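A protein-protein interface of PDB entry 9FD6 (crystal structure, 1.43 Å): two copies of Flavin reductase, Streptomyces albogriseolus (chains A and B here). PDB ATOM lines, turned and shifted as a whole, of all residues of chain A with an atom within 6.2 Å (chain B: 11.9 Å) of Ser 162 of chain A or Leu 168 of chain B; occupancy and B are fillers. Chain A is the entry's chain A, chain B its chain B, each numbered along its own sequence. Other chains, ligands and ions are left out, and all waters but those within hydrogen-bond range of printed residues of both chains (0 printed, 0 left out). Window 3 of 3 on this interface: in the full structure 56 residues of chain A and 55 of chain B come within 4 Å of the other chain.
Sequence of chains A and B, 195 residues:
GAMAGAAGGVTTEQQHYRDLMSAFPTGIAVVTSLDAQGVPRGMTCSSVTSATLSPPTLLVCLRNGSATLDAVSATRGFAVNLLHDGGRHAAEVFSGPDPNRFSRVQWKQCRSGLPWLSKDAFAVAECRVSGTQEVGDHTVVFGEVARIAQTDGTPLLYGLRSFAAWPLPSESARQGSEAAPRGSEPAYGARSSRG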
ATOM      1  N   ARG A  88      -2.469   8.239  41.144  1.00  0.00           N
ATOM      2  CA  ARG A  88      -1.392   8.060  40.177  1.00  0.00           C
ATOM      3  C   ARG A  88      -0.780   6.667  40.267  1.00  0.00           C
ATOM      4  O   ARG A  88      -0.479   6.042  39.244  1.00  0.00           O
ATOM      5  CB  ARG A  88      -0.322   9.123  40.403  1.00  0.00           C
ATOM      6  CG  ARG A  88       0.872   8.936  39.548  1.00  0.00           C
ATOM      7  CD  ARG A  88       1.822  10.092  39.669  1.00  0.00           C
ATOM      8  NE  ARG A  88       2.999   9.831  38.858  1.00  0.00           N
ATOM      9  CZ  ARG A  88       3.939  10.724  38.592  1.00  0.00           C
ATOM     10  NH1 ARG A  88       3.852  11.969  39.032  1.00  0.00           N
ATOM     11  NH2 ARG A  88       4.989  10.359  37.863  1.00  0.00           N
ATOM     12  N   LEU A 157      -5.238  13.898  35.842  1.00  0.00           N
ATOM     13  CA  LEU A 157      -5.080  14.145  34.421  1.00  0.00           C
ATOM     14  C   LEU A 157      -3.798  13.504  33.909  1.00  0.00           C
ATOM     15  O   LEU A 157      -2.848  13.255  34.657  1.00  0.00           O
ATOM     16  CB  LEU A 157      -4.997  15.638  34.099  1.00  0.00           C
ATOM     17  CG  LEU A 157      -6.102  16.562  34.588  1.00  0.00           C
ATOM     18  CD1 LEU A 157      -5.732  18.005  34.229  1.00  0.00           C
ATOM     19  CD2 LEU A 157      -7.438  16.167  33.990  1.00  0.00           C
ATOM     20  N   TYR A 158      -3.774  13.268  32.606  1.00  0.00           N
ATOM     21  CA  TYR A 158      -2.555  12.840  31.943  1.00  0.00           C
ATOM     22  C   TYR A 158      -2.459  13.579  30.622  1.00  0.00           C
ATOM     23  O   TYR A 158      -3.430  13.623  29.861  1.00  0.00           O
ATOM     24  CB  TYR A 158      -2.553  11.334  31.697  1.00  0.00           C
ATOM     25  CG  TYR A 158      -1.197  10.782  31.320  1.00  0.00           C
ATOM     26  CD1 TYR A 158      -0.279  10.433  32.297  1.00  0.00           C
ATOM     27  CD2 TYR A 158      -0.832  10.611  29.991  1.00  0.00           C
ATOM     28  CE1 TYR A 158       0.963   9.922  31.968  1.00  0.00           C
ATOM     29  CE2 TYR A 158       0.415  10.097  29.649  1.00  0.00           C
ATOM     30  CZ  TYR A 158       1.304   9.748  30.646  1.00  0.00           C
ATOM     31  OH  TYR A 158       2.545   9.237  30.325  1.00  0.00           O
ATOM     32  N   GLY A 159      -1.288  14.142  30.355  1.00  0.00           N
ATOM     33  CA  GLY A 159      -1.058  14.889  29.139  1.00  0.00           C
ATOM     34  C   GLY A 159       0.411  15.195  28.986  1.00  0.00           C
ATOM     35  O   GLY A 159       1.126  15.305  29.987  1.00  0.00           O
ATOM     36  N   LEU A 160       0.876  15.327  27.745  1.00  0.00           N
ATOM     37  CA  LEU A 160       2.272  15.668  27.495  1.00  0.00           C
ATOM     38  C   LEU A 160       3.185  14.760  28.316  1.00  0.00           C
ATOM     39  O   LEU A 160       4.151  15.200  28.947  1.00  0.00           O
ATOM     40  CB  LEU A 160       2.529  17.153  27.751  1.00  0.00           C
ATOM     41  CG  LEU A 160       1.817  18.089  26.765  1.00  0.00           C
ATOM     42  CD1 LEU A 160       2.062  19.545  27.159  1.00  0.00           C
ATOM     43  CD2 LEU A 160       2.244  17.831  25.309  1.00  0.00           C
ATOM     44  N   ARG A 161       2.832  13.473  28.331  1.00  0.00           N
ATOM     45  CA  ARG A 161       3.633  12.433  28.966  1.00  0.00           C
ATOM     46  C   ARG A 161       3.819  12.662  30.463  1.00  0.00           C
ATOM     47  O   ARG A 161       4.833  12.255  31.035  1.00  0.00           O
ATOM     48  CB  ARG A 161       4.962  12.248  28.225  1.00  0.00           C
ATOM     49  CG  ARG A 161       4.721  11.884  26.763  1.00  0.00           C
ATOM     50  CD  ARG A 161       5.968  11.883  25.889  1.00  0.00           C
ATOM     51  NE  ARG A 161       5.588  11.530  24.523  1.00  0.00           N
ATOM     52  CZ  ARG A 161       5.846  12.253  23.439  1.00  0.00           C
ATOM     53  NH1 ARG A 161       6.623  13.323  23.486  1.00  0.00           N
ATOM     54  NH2 ARG A 161       5.327  11.879  22.272  1.00  0.00           N
ATOM     55  N   SER A 162       2.846  13.301  31.115  1.00  0.00           N
ATOM     56  CA  SER A 162       2.947  13.579  32.539  1.00  0.00           C
ATOM     57  C   SER A 162       1.579  13.499  33.199  1.00  0.00           C
ATOM     58  O   SER A 162       0.566  13.887  32.608  1.00  0.00           O
ATOM     59  CB  SER A 162       3.529  14.976  32.814  1.00  0.00           C
ATOM     60  OG  SER A 162       3.677  15.206  34.210  1.00  0.00           O
ATOM     61  N   PHE A 163       1.571  13.016  34.438  1.00  0.00           N
ATOM     62  CA  PHE A 163       0.406  13.132  35.299  1.00  0.00           C
ATOM     63  C   PHE A 163       0.319  14.547  35.859  1.00  0.00           C
ATOM     64  O   PHE A 163       1.331  15.219  36.075  1.00  0.00           O
ATOM     65  CB  PHE A 163       0.491  12.150  36.470  1.00  0.00           C
ATOM     66  CG  PHE A 163       0.292  10.728  36.068  1.00  0.00           C
ATOM     67  CD1 PHE A 163      -0.981  10.206  35.912  1.00  0.00           C
ATOM     68  CD2 PHE A 163       1.378   9.912  35.837  1.00  0.00           C
ATOM     69  CE1 PHE A 163      -1.156   8.892  35.525  1.00  0.00           C
ATOM     70  CE2 PHE A 163       1.212   8.605  35.457  1.00  0.00           C
ATOM     71  CZ  PHE A 163      -0.044   8.087  35.300  1.00  0.00           C
ATOM     72  N   ALA A 164      -0.907  14.986  36.106  1.00  0.00           N
ATOM     73  CA  ALA A 164      -1.178  16.262  36.751  1.00  0.00           C
ATOM     74  C   ALA A 164      -2.546  16.141  37.408  1.00  0.00           C
ATOM     75  O   ALA A 164      -3.207  15.105  37.317  1.00  0.00           O
ATOM     76  CB  ALA A 164      -1.119  17.415  35.748  1.00  0.00           C
ATOM     77  N   PRO B  25     -12.003  15.413  32.316  1.00  0.00           N
ATOM     78  CA  PRO B  25     -11.607  16.588  31.528  1.00  0.00           C
ATOM     79  C   PRO B  25     -10.842  16.185  30.276  1.00  0.00           C
ATOM     80  O   PRO B  25     -10.303  15.081  30.169  1.00  0.00           O
ATOM     81  CB  PRO B  25     -10.726  17.395  32.495  1.00  0.00           C
ATOM     82  CG  PRO B  25     -11.095  16.887  33.867  1.00  0.00           C
ATOM     83  CD  PRO B  25     -11.393  15.419  33.657  1.00  0.00           C
ATOM     84  N   GLY B  27      -8.681  17.939  26.504  1.00  0.00           N
ATOM     85  CA  GLY B  27      -8.325  19.023  25.623  1.00  0.00           C
ATOM     86  C   GLY B  27      -9.538  19.450  24.824  1.00  0.00           C
ATOM     87  O   GLY B  27     -10.642  18.924  24.962  1.00  0.00           O
ATOM     88  N   LEU B  83      -6.548  23.343  20.366  1.00  0.00           N
ATOM     89  CA  LEU B  83      -6.499  24.719  20.839  1.00  0.00           C
ATOM     90  C   LEU B  83      -5.507  24.864  21.985  1.00  0.00           C
ATOM     91  O   LEU B  83      -5.472  24.039  22.902  1.00  0.00           O
ATOM     92  CB  LEU B  83      -7.880  25.174  21.309  1.00  0.00           C
ATOM     93  CG  LEU B  83      -8.992  25.186  20.263  1.00  0.00           C
ATOM     94  CD1 LEU B  83     -10.246  25.796  20.871  1.00  0.00           C
ATOM     95  CD2 LEU B  83      -8.557  25.930  19.017  1.00  0.00           C
ATOM     96  N   HIS B  84      -4.695  25.917  21.929  1.00  0.00           N
ATOM     97  CA  HIS B  84      -3.876  26.291  23.070  1.00  0.00           C
ATOM     98  C   HIS B  84      -4.674  27.177  24.033  1.00  0.00           C
ATOM     99  O   HIS B  84      -5.837  27.519  23.799  1.00  0.00           O
ATOM    100  CB  HIS B  84      -2.575  26.952  22.618  1.00  0.00           C
ATOM    101  CG  HIS B  84      -2.774  28.164  21.766  1.00  0.00           C
ATOM    102  ND1 HIS B  84      -3.489  29.263  22.189  1.00  0.00           N
ATOM    103  CD2 HIS B  84      -2.353  28.451  20.513  1.00  0.00           C
ATOM    104  CE1 HIS B  84      -3.494  30.178  21.237  1.00  0.00           C
ATOM    105  NE2 HIS B  84      -2.816  29.707  20.205  1.00  0.00           N
ATOM    106  N   ASP B  85      -4.029  27.562  25.135  1.00  0.00           N
ATOM    107  CA  ASP B  85      -4.730  28.262  26.204  1.00  0.00           C
ATOM    108  C   ASP B  85      -5.249  29.634  25.786  1.00  0.00           C
ATOM    109  O   ASP B  85      -6.154  30.161  26.439  1.00  0.00           O
ATOM    110  CB  ASP B  85      -3.804  28.424  27.406  1.00  0.00           C
ATOM    111  CG  ASP B  85      -2.607  29.296  27.097  1.00  0.00           C
ATOM    112  OD1 ASP B  85      -1.649  28.826  26.446  1.00  0.00           O
ATOM    113  OD2 ASP B  85      -2.646  30.477  27.482  1.00  0.00           O
ATOM    114  N   PHE B 122      -2.401  25.166  18.364  1.00  0.00           N
ATOM    115  CA  PHE B 122      -0.977  24.886  18.347  1.00  0.00           C
ATOM    116  C   PHE B 122      -0.652  23.663  17.507  1.00  0.00           C
ATOM    117  O   PHE B 122       0.522  23.415  17.228  1.00  0.00           O
ATOM    118  CB  PHE B 122      -0.460  24.687  19.775  1.00  0.00           C
ATOM    119  CG  PHE B 122      -0.998  23.460  20.439  1.00  0.00           C
ATOM    120  CD1 PHE B 122      -0.330  22.254  20.329  1.00  0.00           C
ATOM    121  CD2 PHE B 122      -2.174  23.499  21.159  1.00  0.00           C
ATOM    122  CE1 PHE B 122      -0.824  21.112  20.924  1.00  0.00           C
ATOM    123  CE2 PHE B 122      -2.664  22.356  21.764  1.00  0.00           C
ATOM    124  CZ  PHE B 122      -1.996  21.161  21.633  1.00  0.00           C
ATOM    125  N   ASP B 152       4.889  24.108  19.839  1.00  0.00           N
ATOM    126  CA  ASP B 152       4.725  24.079  21.284  1.00  0.00           C
ATOM    127  C   ASP B 152       3.549  24.965  21.683  1.00  0.00           C
ATOM    128  O   ASP B 152       3.221  25.944  21.006  1.00  0.00           O
ATOM    129  CB  ASP B 152       5.995  24.556  21.987  1.00  0.00           C
ATOM    130  CG  ASP B 152       7.120  23.532  21.933  1.00  0.00           C
ATOM    131  OD1 ASP B 152       6.843  22.312  21.920  1.00  0.00           O
ATOM    132  OD2 ASP B 152       8.292  23.957  21.912  1.00  0.00           O
ATOM    133  N   GLY B 153       2.894  24.594  22.771  1.00  0.00           N
ATOM    134  CA  GLY B 153       1.804  25.390  23.299  1.00  0.00           C
ATOM    135  C   GLY B 153       1.197  24.686  24.491  1.00  0.00           C
ATOM    136  O   GLY B 153       1.314  23.465  24.644  1.00  0.00           O
ATOM    137  N   THR B 154       0.567  25.482  25.351  1.00  0.00           N
ATOM    138  CA  THR B 154      -0.128  24.936  26.510  1.00  0.00           C
ATOM    139  C   THR B 154      -1.549  24.584  26.101  1.00  0.00           C
ATOM    140  O   THR B 154      -2.295  25.481  25.683  1.00  0.00           O
ATOM    141  CB  THR B 154      -0.193  25.956  27.634  1.00  0.00           C
ATOM    142  OG1 THR B 154       1.117  26.220  28.141  1.00  0.00           O
ATOM    143  CG2 THR B 154      -1.065  25.424  28.761  1.00  0.00           C
ATOM    144  N   PRO B 155      -1.975  23.324  26.212  1.00  0.00           N
ATOM    145  CA  PRO B 155      -3.328  22.981  25.756  1.00  0.00           C
ATOM    146  C   PRO B 155      -4.417  23.613  26.607  1.00  0.00           C
ATOM    147  O   PRO B 155      -4.324  23.679  27.834  1.00  0.00           O
ATOM    148  CB  PRO B 155      -3.362  21.449  25.848  1.00  0.00           C
ATOM    149  CG  PRO B 155      -1.921  21.041  25.710  1.00  0.00           C
ATOM    150  CD  PRO B 155      -1.148  22.118  26.422  1.00  0.00           C
ATOM    151  N   LEU B 156      -5.452  24.097  25.928  1.00  0.00           N
ATOM    152  CA  LEU B 156      -6.707  24.425  26.582  1.00  0.00           C
ATOM    153  C   LEU B 156      -7.376  23.145  27.076  1.00  0.00           C
ATOM    154  O   LEU B 156      -7.283  22.087  26.448  1.00  0.00           O
ATOM    155  CB  LEU B 156      -7.617  25.121  25.574  1.00  0.00           C
ATOM    156  CG  LEU B 156      -8.947  25.666  26.082  1.00  0.00           C
ATOM    157  CD1 LEU B 156      -8.742  26.785  27.098  1.00  0.00           C
ATOM    158  CD2 LEU B 156      -9.773  26.153  24.905  1.00  0.00           C
ATOM    159  N   LEU B 157      -8.054  23.245  28.217  1.00  0.00           N
ATOM    160  CA  LEU B 157      -8.799  22.130  28.774  1.00  0.00           C
ATOM    161  C   LEU B 157     -10.246  22.542  28.994  1.00  0.00           C
ATOM    162  O   LEU B 157     -10.566  23.727  29.129  1.00  0.00           O
ATOM    163  CB  LEU B 157      -8.243  21.665  30.129  1.00  0.00           C
ATOM    164  CG  LEU B 157      -6.770  21.275  30.210  1.00  0.00           C
ATOM    165  CD1 LEU B 157      -6.389  21.015  31.684  1.00  0.00           C
ATOM    166  CD2 LEU B 157      -6.468  20.070  29.332  1.00  0.00           C
ATOM    167  N   ALA B 164     -10.096  25.591  31.421  1.00  0.00           N
ATOM    168  CA  ALA B 164      -8.884  25.723  32.209  1.00  0.00           C
ATOM    169  C   ALA B 164      -7.709  25.533  31.265  1.00  0.00           C
ATOM    170  O   ALA B 164      -7.883  25.375  30.054  1.00  0.00           O
ATOM    171  CB  ALA B 164      -8.866  24.730  33.371  1.00  0.00           C
ATOM    172  N   ALA B 165      -6.506  25.560  31.824  1.00  0.00           N
ATOM    173  CA  ALA B 165      -5.291  25.376  31.052  1.00  0.00           C
ATOM    174  C   ALA B 165      -4.491  24.222  31.633  1.00  0.00           C
ATOM    175  O   ALA B 165      -4.480  24.007  32.846  1.00  0.00           O
ATOM    176  CB  ALA B 165      -4.418  26.633  31.076  1.00  0.00           C
ATOM    177  N   TRP B 166      -3.818  23.488  30.764  1.00  0.00           N
ATOM    178  CA  TRP B 166      -2.921  22.442  31.229  1.00  0.00           C
ATOM    179  C   TRP B 166      -1.974  23.024  32.281  1.00  0.00           C
ATOM    180  O   TRP B 166      -1.319  24.046  32.024  1.00  0.00           O
ATOM    181  CB  TRP B 166      -2.154  21.868  30.033  1.00  0.00           C
ATOM    182  CG  TRP B 166      -1.153  20.849  30.415  1.00  0.00           C
ATOM    183  CD1 TRP B 166       0.208  20.971  30.352  1.00  0.00           C
ATOM    184  CD2 TRP B 166      -1.414  19.553  30.956  1.00  0.00           C
ATOM    185  NE1 TRP B 166       0.808  19.830  30.819  1.00  0.00           N
ATOM    186  CE2 TRP B 166      -0.164  18.941  31.192  1.00  0.00           C
ATOM    187  CE3 TRP B 166      -2.579  18.846  31.260  1.00  0.00           C
ATOM    188  CZ2 TRP B 166      -0.047  17.660  31.715  1.00  0.00           C
ATOM    189  CZ3 TRP B 166      -2.459  17.568  31.785  1.00  0.00           C
ATOM    190  CH2 TRP B 166      -1.201  16.993  32.009  1.00  0.00           C
ATOM    191  N   PRO B 167      -1.901  22.433  33.479  1.00  0.00           N
ATOM    192  CA  PRO B 167      -1.303  23.137  34.622  1.00  0.00           C
ATOM    193  C   PRO B 167       0.212  23.075  34.720  1.00  0.00           C
ATOM    194  O   PRO B 167       0.769  23.616  35.680  1.00  0.00           O
ATOM    195  CB  PRO B 167      -1.953  22.435  35.828  1.00  0.00           C
ATOM    196  CG  PRO B 167      -2.277  21.072  35.335  1.00  0.00           C
ATOM    197  CD  PRO B 167      -2.636  21.222  33.895  1.00  0.00           C
ATOM    198  N   LEU B 168       0.888  22.458  33.780  1.00  0.00           N
ATOM    199  CA  LEU B 168       2.334  22.359  33.836  1.00  0.00           C
ATOM    200  C   LEU B 168       2.961  23.186  32.721  1.00  0.00           C
ATOM    201  O   LEU B 168       2.397  23.302  31.628  1.00  0.00           O
ATOM    202  CB  LEU B 168       2.775  20.901  33.669  1.00  0.00           C
ATOM    203  CG  LEU B 168       2.205  19.908  34.686  1.00  0.00           C
ATOM    204  CD1 LEU B 168       2.788  18.534  34.457  1.00  0.00           C
ATOM    205  CD2 LEU B 168       2.466  20.370  36.101  1.00  0.00           C
ATOM    206  N   PRO B 169       4.133  23.780  32.967  1.00  0.00           N
ATOM    207  CA  PRO B 169       4.848  24.474  31.890  1.00  0.00           C
ATOM    208  C   PRO B 169       5.398  23.514  30.837  1.00  0.00           C
ATOM    209  O   PRO B 169       5.229  23.804  29.649  1.00  0.00           O
ATOM    210  CB  PRO B 169       5.994  25.174  32.627  1.00  0.00           C
ATOM    211  CG  PRO B 169       6.220  24.358  33.849  1.00  0.00           C
ATOM    212  CD  PRO B 169       4.879  23.793  34.240  1.00  0.00           C
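N of Leu 157 of chain A lies within hydrogen-bond range of O of Ala 164 of chain A, 2.8 Å away. The backbone NH of Trp 166 of chain B is in hydrogen-bond range of the backbone carbonyl oxygen of Pro 155 of chain B (3.0 Å). N of Leu 157 of chain B sits at hydrogen-bond distance from O of Ala 164 of chain B, 2.8 Å away.
Among the printed residues, pairs that only touch across the chains: Gly 159 of chain A with Trp 166 of chain B, Ser 162 of chain A with Leu 168 of chain B, Ser 162 of chain A with Trp 166 of chain B, Leu 157 of chain A with Pro 25 of chain B, Ala 164 of chain A with Trp 166 of chain B, Ala 164 of chain A with Pro 167 of chain B, Leu 160 of chain A with Trp 166 of chain B, Tyr 158 of chain A with Trp 166 of chain B, Leu 157 of chain A with Trp 166 of chain B, Phe 163 of chain A with Leu 168 of chain B and Leu 157 of chain A with Leu 157 of chain B.
Of chain B, only Trp 166 comes within 4 Å of Gly 159 of chain A. Of the printed residues of chain B, Leu 160 of chain A touches Trp 166 (3.9 Å). Of the printed residues of chain B, Ser 162 of chain A touches Trp 166 (3.6 Å) and Leu 168 (3.5 Å). Printed residues of chain B within 4 Å of Phe 163 of chain A: Leu 168 (3.97 Å). Of chain B, only Trp 166 (3.8 Å) and Pro 167 (3.9 Å) come within 4 Å of Ala 164 of chain A. Of the printed residues of chain A, Leu 157 of chain B touches Leu 157. Of the printed residues of chain A, Leu 168 of chain B touches Ser 162 (3.5 Å) and Phe 163 (3.97 Å). The nearest printed residue of chain B that does not touch Ser 162 of chain A is Pro 167 of chain B (8.1 Å).
Of the 18 printed residues of chain B, 5 touch a printed residue of chain A. Printed residues of chain B that touch a printed residue of chain A: Pro 25, Leu 157, Trp 166, Pro 167 and Leu 168. Of the 9 printed residues of chain A, 7 touch a printed residue of chain B. Printed residues of chain A that touch a printed residue of chain B: Leu 157, Tyr 158, Gly 159, Leu 160, Ser 162, Phe 163 and Ala 164. Among the printed residues, 11 pairs touch across the chains.
Leu 157 of chain A touches its own counterpart, Leu 157 of chain B. Positions printed for both chains: 157 and 164.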
